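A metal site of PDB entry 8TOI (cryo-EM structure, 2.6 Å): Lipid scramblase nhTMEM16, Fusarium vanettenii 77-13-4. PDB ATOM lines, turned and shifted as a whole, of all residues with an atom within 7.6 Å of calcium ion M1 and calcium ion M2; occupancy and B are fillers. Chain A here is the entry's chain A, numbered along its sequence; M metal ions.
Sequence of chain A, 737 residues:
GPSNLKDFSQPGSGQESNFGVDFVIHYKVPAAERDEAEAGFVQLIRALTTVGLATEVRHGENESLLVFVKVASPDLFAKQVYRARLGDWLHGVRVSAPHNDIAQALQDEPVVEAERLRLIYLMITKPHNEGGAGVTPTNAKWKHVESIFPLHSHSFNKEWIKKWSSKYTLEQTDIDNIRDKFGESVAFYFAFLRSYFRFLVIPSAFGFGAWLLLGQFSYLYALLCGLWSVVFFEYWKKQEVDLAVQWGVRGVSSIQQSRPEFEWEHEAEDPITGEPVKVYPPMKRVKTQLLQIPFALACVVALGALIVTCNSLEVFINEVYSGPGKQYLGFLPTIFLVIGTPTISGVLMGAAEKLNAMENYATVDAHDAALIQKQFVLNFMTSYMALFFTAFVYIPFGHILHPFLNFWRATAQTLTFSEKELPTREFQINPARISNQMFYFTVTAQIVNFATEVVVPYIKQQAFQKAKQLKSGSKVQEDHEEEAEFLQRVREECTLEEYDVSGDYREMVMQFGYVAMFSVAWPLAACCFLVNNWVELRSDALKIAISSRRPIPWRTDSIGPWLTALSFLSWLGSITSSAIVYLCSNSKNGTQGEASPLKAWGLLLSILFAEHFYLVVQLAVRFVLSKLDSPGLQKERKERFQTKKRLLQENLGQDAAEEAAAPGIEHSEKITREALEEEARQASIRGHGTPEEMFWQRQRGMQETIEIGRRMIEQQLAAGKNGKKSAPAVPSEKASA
Residues that only touch calcium ion M1: Tyr 189 (3.95 Å) and Lys 543 (3.9 Å).
Of the 26 residues printed, 7 come within 4 Å of calcium ion M1.
Calcium ion M1 is bound by OD2 of Asp 540 (2.5 Å), OE2 of Glu 453 (2.6 Å), OE2 of Glu 536 (2.6 Å), OE1 of Glu 507 (2.6 Å), OD1 of Asp 504 (2.7 Å) and OD1 of Asp 540 (2.8 Å).
Calcium ion M1 has six donor atoms within binding distance.
Calcium ion M2 is bound by OE2 of Glu 536 (2.5 Å), OD1 of Asn 449 (2.6 Å), OE1 of Glu 536 (2.6 Å), OE1 of Glu 453 (2.7 Å) and OE2 of Glu 507 (2.8 Å).
OG of Ser 539 lies within hydrogen-bond range of O of Glu 536 (3.4 Å).
The side-chain amino group (NZ) of Lys 543 lies within salt-bridge range of the side-chain carboxylate (OD2) of Asp 504, 3.3 Å away.
The side-chain carboxylate (OD1) of Asp 540 sits close to the side-chain amino group (NZ) of Lys 543 (3.6 Å).
The side-chain amide nitrogen of Asn 532 sits close to the side-chain carboxylate of Glu 536, 3.3 Å away.
OE2 of Glu 453 lies close to NZ of Lys 543, at 2.7 Å.
OH of Tyr 505 sits at hydrogen-bond distance from N of Tyr 189 (3.1 Å).
OH of Tyr 499 sits at hydrogen-bond distance from OD2 of Asp 504, 2.5 Å away.
Four residues have an atom within 4 Å of calcium ion M2: Asn 449, Glu 453, Glu 507 and Glu 536.
The nearest printed residue that does not touch calcium ion M2 is Asn 532 (4.2 Å).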
ATOM      1  N   TYR A 189       9.462  10.674 -15.781  1.00  0.00           N
ATOM      2  CA  TYR A 189      10.460   9.991 -14.963  1.00  0.00           C
ATOM      3  C   TYR A 189      11.527  10.961 -14.454  1.00  0.00           C
ATOM      4  O   TYR A 189      11.911  10.905 -13.277  1.00  0.00           O
ATOM      5  CB  TYR A 189      11.134   8.856 -15.723  1.00  0.00           C
ATOM      6  CG  TYR A 189      12.404   8.389 -15.048  1.00  0.00           C
ATOM      7  CD1 TYR A 189      12.370   7.769 -13.803  1.00  0.00           C
ATOM      8  CD2 TYR A 189      13.636   8.589 -15.653  1.00  0.00           C
ATOM      9  CE1 TYR A 189      13.525   7.374 -13.181  1.00  0.00           C
ATOM     10  CE2 TYR A 189      14.797   8.188 -15.036  1.00  0.00           C
ATOM     11  CZ  TYR A 189      14.730   7.578 -13.798  1.00  0.00           C
ATOM     12  OH  TYR A 189      15.888   7.164 -13.187  1.00  0.00           O
ATOM     13  N   LEU A 193      12.265  11.973 -10.630  1.00  0.00           N
ATOM     14  CA  LEU A 193      13.590  11.787 -10.038  1.00  0.00           C
ATOM     15  C   LEU A 193      14.145  13.097  -9.502  1.00  0.00           C
ATOM     16  O   LEU A 193      14.774  13.109  -8.444  1.00  0.00           O
ATOM     17  CB  LEU A 193      14.529  11.169 -11.074  1.00  0.00           C
ATOM     18  CG  LEU A 193      15.919  10.790 -10.573  1.00  0.00           C
ATOM     19  CD1 LEU A 193      15.840   9.980  -9.308  1.00  0.00           C
ATOM     20  CD2 LEU A 193      16.672  10.023 -11.649  1.00  0.00           C
ATOM     21  N   ALA A 445      24.651  -2.318  -2.232  1.00  0.00           N
ATOM     22  CA  ALA A 445      23.637  -2.172  -3.286  1.00  0.00           C
ATOM     23  C   ALA A 445      23.840  -0.886  -4.078  1.00  0.00           C
ATOM     24  O   ALA A 445      23.327  -0.751  -5.180  1.00  0.00           O
ATOM     25  CB  ALA A 445      22.228  -2.221  -2.706  1.00  0.00           C
ATOM     26  N   GLN A 446      24.573   0.070  -3.509  1.00  0.00           N
ATOM     27  CA  GLN A 446      24.954   1.238  -4.296  1.00  0.00           C
ATOM     28  C   GLN A 446      26.161   0.950  -5.189  1.00  0.00           C
ATOM     29  O   GLN A 446      26.475   1.766  -6.058  1.00  0.00           O
ATOM     30  CB  GLN A 446      25.251   2.425  -3.381  1.00  0.00           C
ATOM     31  CG  GLN A 446      24.028   2.979  -2.660  1.00  0.00           C
ATOM     32  CD  GLN A 446      22.761   2.875  -3.475  1.00  0.00           C
ATOM     33  OE1 GLN A 446      22.570   3.603  -4.442  1.00  0.00           O
ATOM     34  NE2 GLN A 446      21.871   1.962  -3.076  1.00  0.00           N
ATOM     35  N   VAL A 448      26.781  -2.534  -6.659  1.00  0.00           N
ATOM     36  CA  VAL A 448      26.372  -3.482  -7.679  1.00  0.00           C
ATOM     37  C   VAL A 448      25.342  -2.879  -8.636  1.00  0.00           C
ATOM     38  O   VAL A 448      25.367  -3.192  -9.833  1.00  0.00           O
ATOM     39  CB  VAL A 448      25.845  -4.793  -7.049  1.00  0.00           C
ATOM     40  CG1 VAL A 448      26.985  -5.536  -6.372  1.00  0.00           C
ATOM     41  CG2 VAL A 448      24.718  -4.536  -6.058  1.00  0.00           C
ATOM     42  N   ASN A 449      24.476  -1.980  -8.150  1.00  0.00           N
ATOM     43  CA  ASN A 449      23.610  -1.263  -9.067  1.00  0.00           C
ATOM     44  C   ASN A 449      24.391  -0.223  -9.859  1.00  0.00           C
ATOM     45  O   ASN A 449      23.974   0.166 -10.953  1.00  0.00           O
ATOM     46  CB  ASN A 449      22.459  -0.591  -8.307  1.00  0.00           C
ATOM     47  CG  ASN A 449      21.347  -0.147  -9.226  1.00  0.00           C
ATOM     48  OD1 ASN A 449      21.397   0.957  -9.778  1.00  0.00           O
ATOM     49  ND2 ASN A 449      20.340  -0.991  -9.402  1.00  0.00           N
ATOM     50  N   PHE A 450      25.531   0.236  -9.342  1.00  0.00           N
ATOM     51  CA  PHE A 450      26.428   0.996 -10.182  1.00  0.00           C
ATOM     52  C   PHE A 450      27.256   0.082 -11.079  1.00  0.00           C
ATOM     53  O   PHE A 450      27.840   0.553 -12.061  1.00  0.00           O
ATOM     54  CB  PHE A 450      27.350   1.880  -9.338  1.00  0.00           C
ATOM     55  CG  PHE A 450      27.983   2.996 -10.109  1.00  0.00           C
ATOM     56  CD1 PHE A 450      27.237   4.091 -10.509  1.00  0.00           C
ATOM     57  CD2 PHE A 450      29.321   2.937 -10.462  1.00  0.00           C
ATOM     58  CE1 PHE A 450      27.819   5.121 -11.225  1.00  0.00           C
ATOM     59  CE2 PHE A 450      29.914   3.969 -11.170  1.00  0.00           C
ATOM     60  CZ  PHE A 450      29.158   5.060 -11.556  1.00  0.00           C
ATOM     61  N   ALA A 451      27.313  -1.208 -10.771  1.00  0.00           N
ATOM     62  CA  ALA A 451      28.016  -2.142 -11.635  1.00  0.00           C
ATOM     63  C   ALA A 451      27.155  -2.549 -12.814  1.00  0.00           C
ATOM     64  O   ALA A 451      27.492  -2.285 -13.976  1.00  0.00           O
ATOM     65  CB  ALA A 451      28.460  -3.369 -10.834  1.00  0.00           C
ATOM     66  N   GLU A 453      24.444  -1.448 -14.072  1.00  0.00           N
ATOM     67  CA  GLU A 453      23.749  -0.439 -14.856  1.00  0.00           C
ATOM     68  C   GLU A 453      24.678   0.548 -15.550  1.00  0.00           C
ATOM     69  O   GLU A 453      24.284   1.131 -16.560  1.00  0.00           O
ATOM     70  CB  GLU A 453      22.779   0.348 -13.966  1.00  0.00           C
ATOM     71  CG  GLU A 453      21.571   0.917 -14.666  1.00  0.00           C
ATOM     72  CD  GLU A 453      20.730   1.797 -13.760  1.00  0.00           C
ATOM     73  OE1 GLU A 453      21.183   2.102 -12.638  1.00  0.00           O
ATOM     74  OE2 GLU A 453      19.620   2.197 -14.158  1.00  0.00           O
ATOM     75  N   VAL A 454      25.899   0.737 -15.052  1.00  0.00           N
ATOM     76  CA  VAL A 454      26.768   1.773 -15.603  1.00  0.00           C
ATOM     77  C   VAL A 454      28.022   1.187 -16.234  1.00  0.00           C
ATOM     78  O   VAL A 454      28.240   1.331 -17.443  1.00  0.00           O
ATOM     79  CB  VAL A 454      27.143   2.794 -14.520  1.00  0.00           C
ATOM     80  CG1 VAL A 454      28.083   3.839 -15.104  1.00  0.00           C
ATOM     81  CG2 VAL A 454      25.894   3.463 -13.966  1.00  0.00           C
ATOM     82  N   TYR A 499      14.937   1.291 -24.582  1.00  0.00           N
ATOM     83  CA  TYR A 499      14.977   1.838 -23.234  1.00  0.00           C
ATOM     84  C   TYR A 499      13.690   1.549 -22.481  1.00  0.00           C
ATOM     85  O   TYR A 499      12.587   1.784 -23.005  1.00  0.00           O
ATOM     86  CB  TYR A 499      15.230   3.343 -23.273  1.00  0.00           C
ATOM     87  CG  TYR A 499      15.115   4.010 -21.925  1.00  0.00           C
ATOM     88  CD1 TYR A 499      16.031   3.749 -20.922  1.00  0.00           C
ATOM     89  CD2 TYR A 499      14.077   4.889 -21.663  1.00  0.00           C
ATOM     90  CE1 TYR A 499      15.931   4.358 -19.695  1.00  0.00           C
ATOM     91  CE2 TYR A 499      13.971   5.504 -20.429  1.00  0.00           C
ATOM     92  CZ  TYR A 499      14.900   5.228 -19.451  1.00  0.00           C
ATOM     93  OH  TYR A 499      14.792   5.831 -18.224  1.00  0.00           O
ATOM     94  N   ASP A 500      13.817   1.050 -21.261  1.00  0.00           N
ATOM     95  CA  ASP A 500      12.682   0.733 -20.398  1.00  0.00           C
ATOM     96  C   ASP A 500      12.664   1.702 -19.230  1.00  0.00           C
ATOM     97  O   ASP A 500      13.625   1.780 -18.465  1.00  0.00           O
ATOM     98  CB  ASP A 500      12.756  -0.710 -19.905  1.00  0.00           C
ATOM     99  CG  ASP A 500      11.407  -1.254 -19.481  1.00  0.00           C
ATOM    100  OD1 ASP A 500      10.385  -0.672 -19.882  1.00  0.00           O
ATOM    101  OD2 ASP A 500      11.373  -2.261 -18.752  1.00  0.00           O
ATOM    102  N   VAL A 501      11.557   2.432 -19.095  1.00  0.00           N
ATOM    103  CA  VAL A 501      11.422   3.414 -18.023  1.00  0.00           C
ATOM    104  C   VAL A 501      10.913   2.769 -16.733  1.00  0.00           C
ATOM    105  O   VAL A 501      11.154   3.304 -15.638  1.00  0.00           O
ATOM    106  CB  VAL A 501      10.518   4.560 -18.530  1.00  0.00           C
ATOM    107  CG1 VAL A 501       9.077   4.104 -18.714  1.00  0.00           C
ATOM    108  CG2 VAL A 501      10.605   5.775 -17.634  1.00  0.00           C
ATOM    109  N   GLY A 503      11.933   0.021 -15.275  1.00  0.00           N
ATOM    110  CA  GLY A 503      13.024  -0.423 -14.432  1.00  0.00           C
ATOM    111  C   GLY A 503      13.594   0.691 -13.567  1.00  0.00           C
ATOM    112  O   GLY A 503      13.889   0.487 -12.391  1.00  0.00           O
ATOM    113  N   ASP A 504      13.740   1.885 -14.152  1.00  0.00           N
ATOM    114  CA  ASP A 504      14.227   3.034 -13.394  1.00  0.00           C
ATOM    115  C   ASP A 504      13.202   3.502 -12.372  1.00  0.00           C
ATOM    116  O   ASP A 504      13.560   3.881 -11.249  1.00  0.00           O
ATOM    117  CB  ASP A 504      14.588   4.158 -14.352  1.00  0.00           C
ATOM    118  CG  ASP A 504      15.680   3.764 -15.322  1.00  0.00           C
ATOM    119  OD1 ASP A 504      16.569   2.979 -14.935  1.00  0.00           O
ATOM    120  OD2 ASP A 504      15.635   4.232 -16.479  1.00  0.00           O
ATOM    121  N   TYR A 505      11.911   3.476 -12.746  1.00  0.00           N
ATOM    122  CA  TYR A 505      10.840   3.712 -11.786  1.00  0.00           C
ATOM    123  C   TYR A 505      10.876   2.710 -10.639  1.00  0.00           C
ATOM    124  O   TYR A 505      10.695   3.084  -9.485  1.00  0.00           O
ATOM    125  CB  TYR A 505       9.484   3.632 -12.475  1.00  0.00           C
ATOM    126  CG  TYR A 505       9.003   4.896 -13.136  1.00  0.00           C
ATOM    127  CD1 TYR A 505       9.069   6.110 -12.483  1.00  0.00           C
ATOM    128  CD2 TYR A 505       8.439   4.866 -14.405  1.00  0.00           C
ATOM    129  CE1 TYR A 505       8.618   7.264 -13.071  1.00  0.00           C
ATOM    130  CE2 TYR A 505       7.982   6.011 -15.008  1.00  0.00           C
ATOM    131  CZ  TYR A 505       8.070   7.211 -14.334  1.00  0.00           C
ATOM    132  OH  TYR A 505       7.613   8.357 -14.937  1.00  0.00           O
ATOM    133  N   GLU A 507      13.539   1.025  -9.536  1.00  0.00           N
ATOM    134  CA  GLU A 507      14.710   1.286  -8.709  1.00  0.00           C
ATOM    135  C   GLU A 507      14.476   2.457  -7.761  1.00  0.00           C
ATOM    136  O   GLU A 507      14.813   2.379  -6.567  1.00  0.00           O
ATOM    137  CB  GLU A 507      15.922   1.553  -9.603  1.00  0.00           C
ATOM    138  CG  GLU A 507      17.216   1.758  -8.849  1.00  0.00           C
ATOM    139  CD  GLU A 507      18.301   2.355  -9.711  1.00  0.00           C
ATOM    140  OE1 GLU A 507      18.160   2.312 -10.955  1.00  0.00           O
ATOM    141  OE2 GLU A 507      19.284   2.886  -9.161  1.00  0.00           O
ATOM    142  N   MET A 508      13.841   3.529  -8.247  1.00  0.00           N
ATOM    143  CA  MET A 508      13.557   4.654  -7.366  1.00  0.00           C
ATOM    144  C   MET A 508      12.460   4.342  -6.359  1.00  0.00           C
ATOM    145  O   MET A 508      12.501   4.856  -5.230  1.00  0.00           O
ATOM    146  CB  MET A 508      13.220   5.892  -8.187  1.00  0.00           C
ATOM    147  CG  MET A 508      14.424   6.421  -8.925  1.00  0.00           C
ATOM    148  SD  MET A 508      15.810   6.673  -7.798  1.00  0.00           S
ATOM    149  CE  MET A 508      17.038   5.580  -8.490  1.00  0.00           C
ATOM    150  N   GLN A 511      14.203   2.425  -3.649  1.00  0.00           N
ATOM    151  CA  GLN A 511      14.980   3.354  -2.837  1.00  0.00           C
ATOM    152  C   GLN A 511      14.100   4.132  -1.865  1.00  0.00           C
ATOM    153  O   GLN A 511      14.467   4.331  -0.698  1.00  0.00           O
ATOM    154  CB  GLN A 511      15.744   4.311  -3.751  1.00  0.00           C
ATOM    155  CG  GLN A 511      16.828   5.077  -3.050  1.00  0.00           C
ATOM    156  CD  GLN A 511      17.651   5.876  -4.010  1.00  0.00           C
ATOM    157  OE1 GLN A 511      18.505   5.343  -4.711  1.00  0.00           O
ATOM    158  NE2 GLN A 511      17.391   7.182  -4.072  1.00  0.00           N
ATOM    159  N   ASN A 532      23.514   9.354  -4.671  1.00  0.00           N
ATOM    160  CA  ASN A 532      23.210   8.439  -5.757  1.00  0.00           C
ATOM    161  C   ASN A 532      22.208   9.041  -6.724  1.00  0.00           C
ATOM    162  O   ASN A 532      22.368   8.898  -7.937  1.00  0.00           O
ATOM    163  CB  ASN A 532      22.688   7.112  -5.197  1.00  0.00           C
ATOM    164  CG  ASN A 532      22.218   6.166  -6.279  1.00  0.00           C
ATOM    165  OD1 ASN A 532      23.030   5.572  -6.986  1.00  0.00           O
ATOM    166  ND2 ASN A 532      20.910   6.045  -6.424  1.00  0.00           N
ATOM    167  N   VAL A 535      23.838  11.263  -9.122  1.00  0.00           N
ATOM    168  CA  VAL A 535      24.419  10.508 -10.215  1.00  0.00           C
ATOM    169  C   VAL A 535      23.337  10.023 -11.145  1.00  0.00           C
ATOM    170  O   VAL A 535      23.497  10.080 -12.381  1.00  0.00           O
ATOM    171  CB  VAL A 535      25.279   9.350  -9.663  1.00  0.00           C
ATOM    172  CG1 VAL A 535      25.985   8.616 -10.789  1.00  0.00           C
ATOM    173  CG2 VAL A 535      26.295   9.884  -8.672  1.00  0.00           C
ATOM    174  N   GLU A 536      22.183   9.624 -10.592  1.00  0.00           N
ATOM    175  CA  GLU A 536      21.178   8.875 -11.347  1.00  0.00           C
ATOM    176  C   GLU A 536      20.554   9.734 -12.437  1.00  0.00           C
ATOM    177  O   GLU A 536      20.477   9.303 -13.592  1.00  0.00           O
ATOM    178  CB  GLU A 536      20.107   8.336 -10.410  1.00  0.00           C
ATOM    179  CG  GLU A 536      19.386   7.112 -10.937  1.00  0.00           C
ATOM    180  CD  GLU A 536      20.143   5.833 -10.676  1.00  0.00           C
ATOM    181  OE1 GLU A 536      20.978   5.817  -9.751  1.00  0.00           O
ATOM    182  OE2 GLU A 536      19.898   4.841 -11.385  1.00  0.00           O
ATOM    183  N   LEU A 537      20.199  10.982 -12.095  1.00  0.00           N
ATOM    184  CA  LEU A 537      19.683  11.969 -13.048  1.00  0.00           C
ATOM    185  C   LEU A 537      20.628  12.196 -14.214  1.00  0.00           C
ATOM    186  O   LEU A 537      20.178  12.515 -15.311  1.00  0.00           O
ATOM    187  CB  LEU A 537      19.441  13.302 -12.342  1.00  0.00           C
ATOM    188  CG  LEU A 537      18.112  13.585 -11.659  1.00  0.00           C
ATOM    189  CD1 LEU A 537      18.244  14.756 -10.719  1.00  0.00           C
ATOM    190  CD2 LEU A 537      17.033  13.832 -12.695  1.00  0.00           C
ATOM    191  N   SER A 539      23.178   9.669 -14.936  1.00  0.00           N
ATOM    192  CA  SER A 539      23.637   8.383 -15.465  1.00  0.00           C
ATOM    193  C   SER A 539      22.554   7.709 -16.295  1.00  0.00           C
ATOM    194  O   SER A 539      22.835   7.200 -17.390  1.00  0.00           O
ATOM    195  CB  SER A 539      24.091   7.462 -14.337  1.00  0.00           C
ATOM    196  OG  SER A 539      22.994   7.085 -13.531  1.00  0.00           O
ATOM    197  N   ASP A 540      21.318   7.737 -15.804  1.00  0.00           N
ATOM    198  CA  ASP A 540      20.174   7.289 -16.598  1.00  0.00           C
ATOM    199  C   ASP A 540      20.018   8.127 -17.851  1.00  0.00           C
ATOM    200  O   ASP A 540      19.637   7.590 -18.898  1.00  0.00           O
ATOM    201  CB  ASP A 540      18.892   7.350 -15.765  1.00  0.00           C
ATOM    202  CG  ASP A 540      18.820   6.236 -14.737  1.00  0.00           C
ATOM    203  OD1 ASP A 540      19.680   5.341 -14.768  1.00  0.00           O
ATOM    204  OD2 ASP A 540      17.891   6.263 -13.902  1.00  0.00           O
ATOM    205  N   LYS A 543      22.248   6.667 -20.025  1.00  0.00           N
ATOM    206  CA  LYS A 543      21.663   5.405 -20.465  1.00  0.00           C
ATOM    207  C   LYS A 543      20.721   5.616 -21.639  1.00  0.00           C
ATOM    208  O   LYS A 543      20.516   4.714 -22.456  1.00  0.00           O
ATOM    209  CB  LYS A 543      20.936   4.727 -19.295  1.00  0.00           C
ATOM    210  CG  LYS A 543      20.645   3.259 -19.508  1.00  0.00           C
ATOM    211  CD  LYS A 543      20.196   2.603 -18.221  1.00  0.00           C
ATOM    212  CE  LYS A 543      18.901   3.204 -17.723  1.00  0.00           C
ATOM    213  NZ  LYS A 543      18.373   2.447 -16.559  1.00  0.00           N
HETATM  214 CA    CA M   1      18.118   3.906 -12.980  1.00  0.00          CA
HETATM  215 CA    CA M   2      21.730   3.425 -10.336  1.00  0.00          CA
